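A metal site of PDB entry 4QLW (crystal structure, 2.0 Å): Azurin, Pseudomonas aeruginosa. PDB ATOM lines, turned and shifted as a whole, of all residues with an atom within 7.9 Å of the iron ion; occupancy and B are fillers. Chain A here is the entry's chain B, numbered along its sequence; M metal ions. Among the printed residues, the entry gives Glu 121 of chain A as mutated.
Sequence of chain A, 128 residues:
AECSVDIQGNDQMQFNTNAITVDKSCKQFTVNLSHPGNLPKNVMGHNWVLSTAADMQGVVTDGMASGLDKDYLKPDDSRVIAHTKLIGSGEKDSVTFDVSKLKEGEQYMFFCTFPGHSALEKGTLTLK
Merely in contact with the iron ion: Gly 45 (3.0 Å). Along chain A the residues within 4 Å of the iron ion span positions 45 to 121. The nearest printed residue that does not touch the iron ion is Phe 114 (4.2 Å).
A ring nitrogen (NE2) of His 46 lies close to the backbone carbonyl oxygen of Gly 9. A ring nitrogen (NE2) of His 117 lies close to the side-chain sulfur (SD) of Met 44 (3.6 Å). The side-chain sulfur of Cys 112 lies close to the backbone carbonyl oxygen of Gly 45 (3.7 Å). O of His 46 sits at hydrogen-bond distance from N of Ile 87. A ring nitrogen (NE2) of His 46 is in hydrogen-bond range of the backbone carbonyl oxygen of Asn 10, 2.7 Å away. The backbone carbonyl oxygen of Gly 45 sits close to a ring nitrogen (ND1) of His 117 (3.3 Å). N of Asn 47 sits close to SG of Cys 112 (3.4 Å). SG of Cys 112 lies close to N of Phe 114.
The iron ion is bound by the side-chain carboxylate (OE1) of Glu 121 (1.9 Å), a ring nitrogen (ND1) of His 46 (2.1 Å), a ring nitrogen (ND1) of His 117 (2.1 Å) and the side-chain sulfur (SG) of Cys 112 (2.4 Å).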
ATOM      1  N   GLY A   9      17.570 -33.984 -25.277  1.00  0.00           N
ATOM      2  CA  GLY A   9      16.731 -33.825 -26.510  1.00  0.00           C
ATOM      3  C   GLY A   9      17.450 -34.571 -27.601  1.00  0.00           C
ATOM      4  O   GLY A   9      18.649 -34.367 -27.807  1.00  0.00           O
ATOM      5  N   ASN A  10      16.755 -35.452 -28.312  1.00  0.00           N
ATOM      6  CA  ASN A  10      17.491 -36.338 -29.217  1.00  0.00           C
ATOM      7  C   ASN A  10      17.207 -36.084 -30.670  1.00  0.00           C
ATOM      8  O   ASN A  10      16.795 -34.970 -31.011  1.00  0.00           O
ATOM      9  CB  ASN A  10      17.231 -37.822 -28.822  1.00  0.00           C
ATOM     10  CG  ASN A  10      15.829 -38.304 -29.178  1.00  0.00           C
ATOM     11  OD1 ASN A  10      14.853 -37.519 -29.256  1.00  0.00           O
ATOM     12  ND2 ASN A  10      15.718 -39.616 -29.411  1.00  0.00           N
ATOM     13  N   MET A  13      13.348 -35.418 -31.914  1.00  0.00           N
ATOM     14  CA  MET A  13      12.659 -34.194 -31.582  1.00  0.00           C
ATOM     15  C   MET A  13      11.726 -34.437 -30.401  1.00  0.00           C
ATOM     16  O   MET A  13      10.529 -34.099 -30.428  1.00  0.00           O
ATOM     17  CB  MET A  13      11.957 -33.655 -32.861  1.00  0.00           C
ATOM     18  CG  MET A  13      11.255 -32.311 -32.741  1.00  0.00           C
ATOM     19  SD  MET A  13      10.314 -31.785 -34.208  1.00  0.00           S
ATOM     20  CE  MET A  13       8.794 -32.562 -33.713  1.00  0.00           C
ATOM     21  N   GLN A  14      12.284 -35.014 -29.329  1.00  0.00           N
ATOM     22  CA  GLN A  14      11.594 -35.057 -28.025  1.00  0.00           C
ATOM     23  C   GLN A  14      12.590 -34.851 -26.890  1.00  0.00           C
ATOM     24  O   GLN A  14      13.772 -35.179 -27.040  1.00  0.00           O
ATOM     25  CB  GLN A  14      10.896 -36.409 -27.765  1.00  0.00           C
ATOM     26  CG  GLN A  14       9.804 -36.768 -28.764  1.00  0.00           C
ATOM     27  CD  GLN A  14       9.066 -38.084 -28.436  1.00  0.00           C
ATOM     28  OE1 GLN A  14       9.536 -38.929 -27.661  1.00  0.00           O
ATOM     29  NE2 GLN A  14       7.877 -38.236 -29.017  1.00  0.00           N
ATOM     30  N   PHE A  15      12.103 -34.313 -25.787  1.00  0.00           N
ATOM     31  CA  PHE A  15      12.798 -34.250 -24.533  1.00  0.00           C
ATOM     32  C   PHE A  15      12.437 -35.496 -23.760  1.00  0.00           C
ATOM     33  O   PHE A  15      11.353 -36.036 -23.934  1.00  0.00           O
ATOM     34  CB  PHE A  15      12.271 -33.105 -23.677  1.00  0.00           C
ATOM     35  CG  PHE A  15      12.791 -31.726 -24.066  1.00  0.00           C
ATOM     36  CD1 PHE A  15      14.023 -31.552 -24.727  1.00  0.00           C
ATOM     37  CD2 PHE A  15      12.059 -30.597 -23.704  1.00  0.00           C
ATOM     38  CE1 PHE A  15      14.483 -30.274 -25.061  1.00  0.00           C
ATOM     39  CE2 PHE A  15      12.535 -29.322 -24.027  1.00  0.00           C
ATOM     40  CZ  PHE A  15      13.736 -29.171 -24.700  1.00  0.00           C
ATOM     41  N   LEU A  33      21.446 -29.642 -20.135  1.00  0.00           N
ATOM     42  CA  LEU A  33      20.920 -30.148 -21.415  1.00  0.00           C
ATOM     43  C   LEU A  33      21.963 -30.865 -22.243  1.00  0.00           C
ATOM     44  O   LEU A  33      23.033 -30.325 -22.467  1.00  0.00           O
ATOM     45  CB  LEU A  33      20.306 -28.992 -22.208  1.00  0.00           C
ATOM     46  CG  LEU A  33      19.525 -29.324 -23.471  1.00  0.00           C
ATOM     47  CD1 LEU A  33      18.185 -29.984 -23.117  1.00  0.00           C
ATOM     48  CD2 LEU A  33      19.318 -28.033 -24.251  1.00  0.00           C
ATOM     49  N   HIS A  35      22.340 -33.489 -25.975  1.00  0.00           N
ATOM     50  CA  HIS A  35      21.737 -33.918 -27.216  1.00  0.00           C
ATOM     51  C   HIS A  35      22.345 -35.267 -27.740  1.00  0.00           C
ATOM     52  O   HIS A  35      23.290 -35.290 -28.568  1.00  0.00           O
ATOM     53  CB  HIS A  35      21.844 -32.754 -28.166  1.00  0.00           C
ATOM     54  CG  HIS A  35      21.166 -32.962 -29.508  1.00  0.00           C
ATOM     55  ND1 HIS A  35      20.806 -34.185 -29.951  1.00  0.00           N
ATOM     56  CD2 HIS A  35      20.785 -32.042 -30.494  1.00  0.00           C
ATOM     57  CE1 HIS A  35      20.236 -34.062 -31.195  1.00  0.00           C
ATOM     58  NE2 HIS A  35      20.216 -32.734 -31.507  1.00  0.00           N
ATOM     59  N   VAL A  43      19.645 -28.717 -38.240  1.00  0.00           N
ATOM     60  CA  VAL A  43      18.480 -29.539 -38.616  1.00  0.00           C
ATOM     61  C   VAL A  43      17.675 -29.897 -37.377  1.00  0.00           C
ATOM     62  O   VAL A  43      16.465 -30.033 -37.432  1.00  0.00           O
ATOM     63  CB  VAL A  43      18.941 -30.834 -39.326  1.00  0.00           C
ATOM     64  CG1 VAL A  43      17.787 -31.810 -39.473  1.00  0.00           C
ATOM     65  CG2 VAL A  43      19.603 -30.537 -40.687  1.00  0.00           C
ATOM     66  N   MET A  44      18.366 -30.134 -36.281  1.00  0.00           N
ATOM     67  CA  MET A  44      17.759 -30.665 -35.044  1.00  0.00           C
ATOM     68  C   MET A  44      18.346 -30.024 -33.795  1.00  0.00           C
ATOM     69  O   MET A  44      18.722 -30.734 -32.837  1.00  0.00           O
ATOM     70  CB  MET A  44      17.933 -32.220 -34.934  1.00  0.00           C
ATOM     71  CG  MET A  44      17.064 -32.918 -33.824  1.00  0.00           C
ATOM     72  SD  MET A  44      15.240 -32.707 -33.909  1.00  0.00           S
ATOM     73  CE  MET A  44      14.893 -33.616 -35.440  1.00  0.00           C
ATOM     74  N   GLY A  45      18.445 -28.706 -33.797  1.00  0.00           N
ATOM     75  CA  GLY A  45      18.893 -27.940 -32.606  1.00  0.00           C
ATOM     76  C   GLY A  45      17.911 -28.048 -31.438  1.00  0.00           C
ATOM     77  O   GLY A  45      16.654 -28.089 -31.605  1.00  0.00           O
ATOM     78  N   HIS A  46      18.476 -28.140 -30.234  1.00  0.00           N
ATOM     79  CA  HIS A  46      17.642 -28.037 -29.050  1.00  0.00           C
ATOM     80  C   HIS A  46      18.169 -26.971 -28.106  1.00  0.00           C
ATOM     81  O   HIS A  46      19.400 -26.753 -27.978  1.00  0.00           O
ATOM     82  CB  HIS A  46      17.560 -29.345 -28.255  1.00  0.00           C
ATOM     83  CG  HIS A  46      16.990 -30.502 -29.023  1.00  0.00           C
ATOM     84  ND1 HIS A  46      15.783 -30.462 -29.669  1.00  0.00           N
ATOM     85  CD2 HIS A  46      17.508 -31.802 -29.221  1.00  0.00           C
ATOM     86  CE1 HIS A  46      15.554 -31.653 -30.249  1.00  0.00           C
ATOM     87  NE2 HIS A  46      16.627 -32.479 -29.942  1.00  0.00           N
ATOM     88  N   ASN A  47      17.252 -26.251 -27.468  1.00  0.00           N
ATOM     89  CA  ASN A  47      17.608 -25.409 -26.307  1.00  0.00           C
ATOM     90  C   ASN A  47      16.602 -25.749 -25.235  1.00  0.00           C
ATOM     91  O   ASN A  47      15.606 -26.475 -25.502  1.00  0.00           O
ATOM     92  CB  ASN A  47      17.673 -23.887 -26.621  1.00  0.00           C
ATOM     93  CG  ASN A  47      16.435 -23.322 -27.379  1.00  0.00           C
ATOM     94  OD1 ASN A  47      15.377 -23.941 -27.459  1.00  0.00           O
ATOM     95  ND2 ASN A  47      16.593 -22.106 -27.924  1.00  0.00           N
ATOM     96  N   TRP A  48      16.832 -25.224 -24.033  1.00  0.00           N
ATOM     97  CA  TRP A  48      15.850 -25.291 -22.965  1.00  0.00           C
ATOM     98  C   TRP A  48      15.583 -23.878 -22.543  1.00  0.00           C
ATOM     99  O   TRP A  48      16.521 -23.109 -22.145  1.00  0.00           O
ATOM    100  CB  TRP A  48      16.373 -26.127 -21.815  1.00  0.00           C
ATOM    101  CG  TRP A  48      15.408 -26.335 -20.690  1.00  0.00           C
ATOM    102  CD1 TRP A  48      14.577 -27.450 -20.477  1.00  0.00           C
ATOM    103  CD2 TRP A  48      15.168 -25.456 -19.534  1.00  0.00           C
ATOM    104  NE1 TRP A  48      13.860 -27.316 -19.299  1.00  0.00           N
ATOM    105  CE2 TRP A  48      14.200 -26.159 -18.675  1.00  0.00           C
ATOM    106  CE3 TRP A  48      15.632 -24.197 -19.132  1.00  0.00           C
ATOM    107  CZ2 TRP A  48      13.706 -25.581 -17.518  1.00  0.00           C
ATOM    108  CZ3 TRP A  48      15.173 -23.671 -17.929  1.00  0.00           C
ATOM    109  CH2 TRP A  48      14.222 -24.332 -17.142  1.00  0.00           C
ATOM    110  N   LEU A  86      21.447 -23.012 -27.840  1.00  0.00           N
ATOM    111  CA  LEU A  86      20.985 -24.019 -28.780  1.00  0.00           C
ATOM    112  C   LEU A  86      22.141 -24.984 -29.024  1.00  0.00           C
ATOM    113  O   LEU A  86      23.252 -24.558 -29.384  1.00  0.00           O
ATOM    114  CB  LEU A  86      20.587 -23.333 -30.072  1.00  0.00           C
ATOM    115  CG  LEU A  86      19.821 -24.163 -31.086  1.00  0.00           C
ATOM    116  CD1 LEU A  86      18.363 -24.397 -30.694  1.00  0.00           C
ATOM    117  CD2 LEU A  86      19.897 -23.553 -32.507  1.00  0.00           C
ATOM    118  N   ILE A  87      21.900 -26.269 -28.820  1.00  0.00           N
ATOM    119  CA  ILE A  87      22.942 -27.291 -29.031  1.00  0.00           C
ATOM    120  C   ILE A  87      22.545 -28.295 -30.122  1.00  0.00           C
ATOM    121  O   ILE A  87      21.316 -28.497 -30.453  1.00  0.00           O
ATOM    122  CB  ILE A  87      23.290 -28.062 -27.751  1.00  0.00           C
ATOM    123  CG1 ILE A  87      22.040 -28.741 -27.172  1.00  0.00           C
ATOM    124  CG2 ILE A  87      24.064 -27.178 -26.793  1.00  0.00           C
ATOM    125  CD1 ILE A  87      22.344 -29.732 -26.064  1.00  0.00           C
ATOM    126  N   PHE A 111      10.533 -25.307 -22.755  1.00  0.00           N
ATOM    127  CA  PHE A 111      10.324 -25.635 -24.190  1.00  0.00           C
ATOM    128  C   PHE A 111      11.599 -25.369 -25.026  1.00  0.00           C
ATOM    129  O   PHE A 111      12.518 -24.611 -24.637  1.00  0.00           O
ATOM    130  CB  PHE A 111       9.102 -24.880 -24.774  1.00  0.00           C
ATOM    131  CG  PHE A 111       9.091 -23.388 -24.433  1.00  0.00           C
ATOM    132  CD1 PHE A 111       9.796 -22.462 -25.218  1.00  0.00           C
ATOM    133  CD2 PHE A 111       8.462 -22.936 -23.295  1.00  0.00           C
ATOM    134  CE1 PHE A 111       9.843 -21.096 -24.896  1.00  0.00           C
ATOM    135  CE2 PHE A 111       8.489 -21.602 -22.967  1.00  0.00           C
ATOM    136  CZ  PHE A 111       9.175 -20.684 -23.743  1.00  0.00           C
ATOM    137  N   CYS A 112      11.672 -26.001 -26.177  1.00  0.00           N
ATOM    138  CA  CYS A 112      12.703 -25.674 -27.126  1.00  0.00           C
ATOM    139  C   CYS A 112      12.129 -24.697 -28.173  1.00  0.00           C
ATOM    140  O   CYS A 112      10.985 -24.852 -28.622  1.00  0.00           O
ATOM    141  CB  CYS A 112      13.137 -27.002 -27.765  1.00  0.00           C
ATOM    142  SG  CYS A 112      14.300 -26.770 -29.111  1.00  0.00           S
ATOM    143  N   THR A 113      12.886 -23.692 -28.604  1.00  0.00           N
ATOM    144  CA  THR A 113      12.322 -22.761 -29.604  1.00  0.00           C
ATOM    145  C   THR A 113      12.739 -23.034 -31.062  1.00  0.00           C
ATOM    146  O   THR A 113      12.360 -22.257 -31.931  1.00  0.00           O
ATOM    147  CB  THR A 113      12.667 -21.268 -29.326  1.00  0.00           C
ATOM    148  OG1 THR A 113      14.080 -21.126 -29.302  1.00  0.00           O
ATOM    149  CG2 THR A 113      12.114 -20.760 -28.020  1.00  0.00           C
ATOM    150  N   PHE A 114      13.516 -24.107 -31.336  1.00  0.00           N
ATOM    151  CA  PHE A 114      13.827 -24.496 -32.711  1.00  0.00           C
ATOM    152  C   PHE A 114      12.480 -24.677 -33.459  1.00  0.00           C
ATOM    153  O   PHE A 114      11.538 -25.173 -32.893  1.00  0.00           O
ATOM    154  CB  PHE A 114      14.644 -25.829 -32.693  1.00  0.00           C
ATOM    155  CG  PHE A 114      15.327 -26.146 -33.997  1.00  0.00           C
ATOM    156  CD1 PHE A 114      16.607 -25.634 -34.270  1.00  0.00           C
ATOM    157  CD2 PHE A 114      14.675 -26.872 -34.982  1.00  0.00           C
ATOM    158  CE1 PHE A 114      17.218 -25.928 -35.497  1.00  0.00           C
ATOM    159  CE2 PHE A 114      15.292 -27.088 -36.222  1.00  0.00           C
ATOM    160  CZ  PHE A 114      16.568 -26.668 -36.433  1.00  0.00           C
ATOM    161  N   PRO A 115      12.362 -24.207 -34.722  1.00  0.00           N
ATOM    162  CA  PRO A 115      11.016 -24.209 -35.330  1.00  0.00           C
ATOM    163  C   PRO A 115      10.283 -25.546 -35.286  1.00  0.00           C
ATOM    164  O   PRO A 115      10.816 -26.597 -35.642  1.00  0.00           O
ATOM    165  CB  PRO A 115      11.296 -23.778 -36.782  1.00  0.00           C
ATOM    166  CG  PRO A 115      12.523 -22.900 -36.636  1.00  0.00           C
ATOM    167  CD  PRO A 115      13.357 -23.504 -35.548  1.00  0.00           C
ATOM    168  N   GLY A 116       9.061 -25.488 -34.798  1.00  0.00           N
ATOM    169  CA  GLY A 116       8.143 -26.604 -34.707  1.00  0.00           C
ATOM    170  C   GLY A 116       8.394 -27.476 -33.499  1.00  0.00           C
ATOM    171  O   GLY A 116       7.540 -28.336 -33.167  1.00  0.00           O
ATOM    172  N   HIS A 117       9.536 -27.334 -32.831  1.00  0.00           N
ATOM    173  CA  HIS A 117       9.843 -28.393 -31.813  1.00  0.00           C
ATOM    174  C   HIS A 117       8.946 -28.338 -30.653  1.00  0.00           C
ATOM    175  O   HIS A 117       8.759 -29.343 -29.952  1.00  0.00           O
ATOM    176  CB  HIS A 117      11.287 -28.292 -31.263  1.00  0.00           C
ATOM    177  CG  HIS A 117      12.311 -28.814 -32.226  1.00  0.00           C
ATOM    178  ND1 HIS A 117      13.573 -29.172 -31.849  1.00  0.00           N
ATOM    179  CD2 HIS A 117      12.209 -29.051 -33.588  1.00  0.00           C
ATOM    180  CE1 HIS A 117      14.243 -29.603 -32.899  1.00  0.00           C
ATOM    181  NE2 HIS A 117      13.401 -29.558 -33.985  1.00  0.00           N
ATOM    182  N   SER A 118       8.411 -27.153 -30.376  1.00  0.00           N
ATOM    183  CA  SER A 118       7.821 -26.993 -29.042  1.00  0.00           C
ATOM    184  C   SER A 118       6.485 -27.702 -28.921  1.00  0.00           C
ATOM    185  O   SER A 118       6.001 -28.008 -27.792  1.00  0.00           O
ATOM    186  CB  SER A 118       7.673 -25.514 -28.714  1.00  0.00           C
ATOM    187  OG  SER A 118       6.671 -24.958 -29.502  1.00  0.00           O
ATOM    188  N   LEU A 120       6.086 -30.720 -29.266  1.00  0.00           N
ATOM    189  CA  LEU A 120       6.411 -31.953 -28.543  1.00  0.00           C
ATOM    190  C   LEU A 120       7.400 -31.687 -27.458  1.00  0.00           C
ATOM    191  O   LEU A 120       7.343 -32.320 -26.397  1.00  0.00           O
ATOM    192  CB  LEU A 120       7.086 -32.929 -29.500  1.00  0.00           C
ATOM    193  CG  LEU A 120       6.298 -33.489 -30.685  1.00  0.00           C
ATOM    194  CD1 LEU A 120       7.082 -34.755 -31.004  1.00  0.00           C
ATOM    195  CD2 LEU A 120       4.819 -33.763 -30.379  1.00  0.00           C
ATOM    196  N   GLU A 121       8.350 -30.802 -27.729  1.00  0.00           N
ATOM    197  CA  GLU A 121       9.430 -30.478 -26.735  1.00  0.00           C
ATOM    198  C   GLU A 121       9.078 -29.312 -25.776  1.00  0.00           C
ATOM    199  O   GLU A 121       9.447 -28.154 -26.032  1.00  0.00           O
ATOM    200  CB  GLU A 121      10.691 -30.137 -27.501  1.00  0.00           C
ATOM    201  CG  GLU A 121      11.351 -31.386 -28.103  1.00  0.00           C
ATOM    202  CD  GLU A 121      12.516 -30.961 -28.982  1.00  0.00           C
ATOM    203  OE1 GLU A 121      13.171 -29.959 -28.733  1.00  0.00           O
ATOM    204  OE2 GLU A 121      12.757 -31.589 -30.003  1.00  0.00           O
HETATM  205 FE    FE M   1      14.361 -29.000 -29.934  1.00  0.00          FE
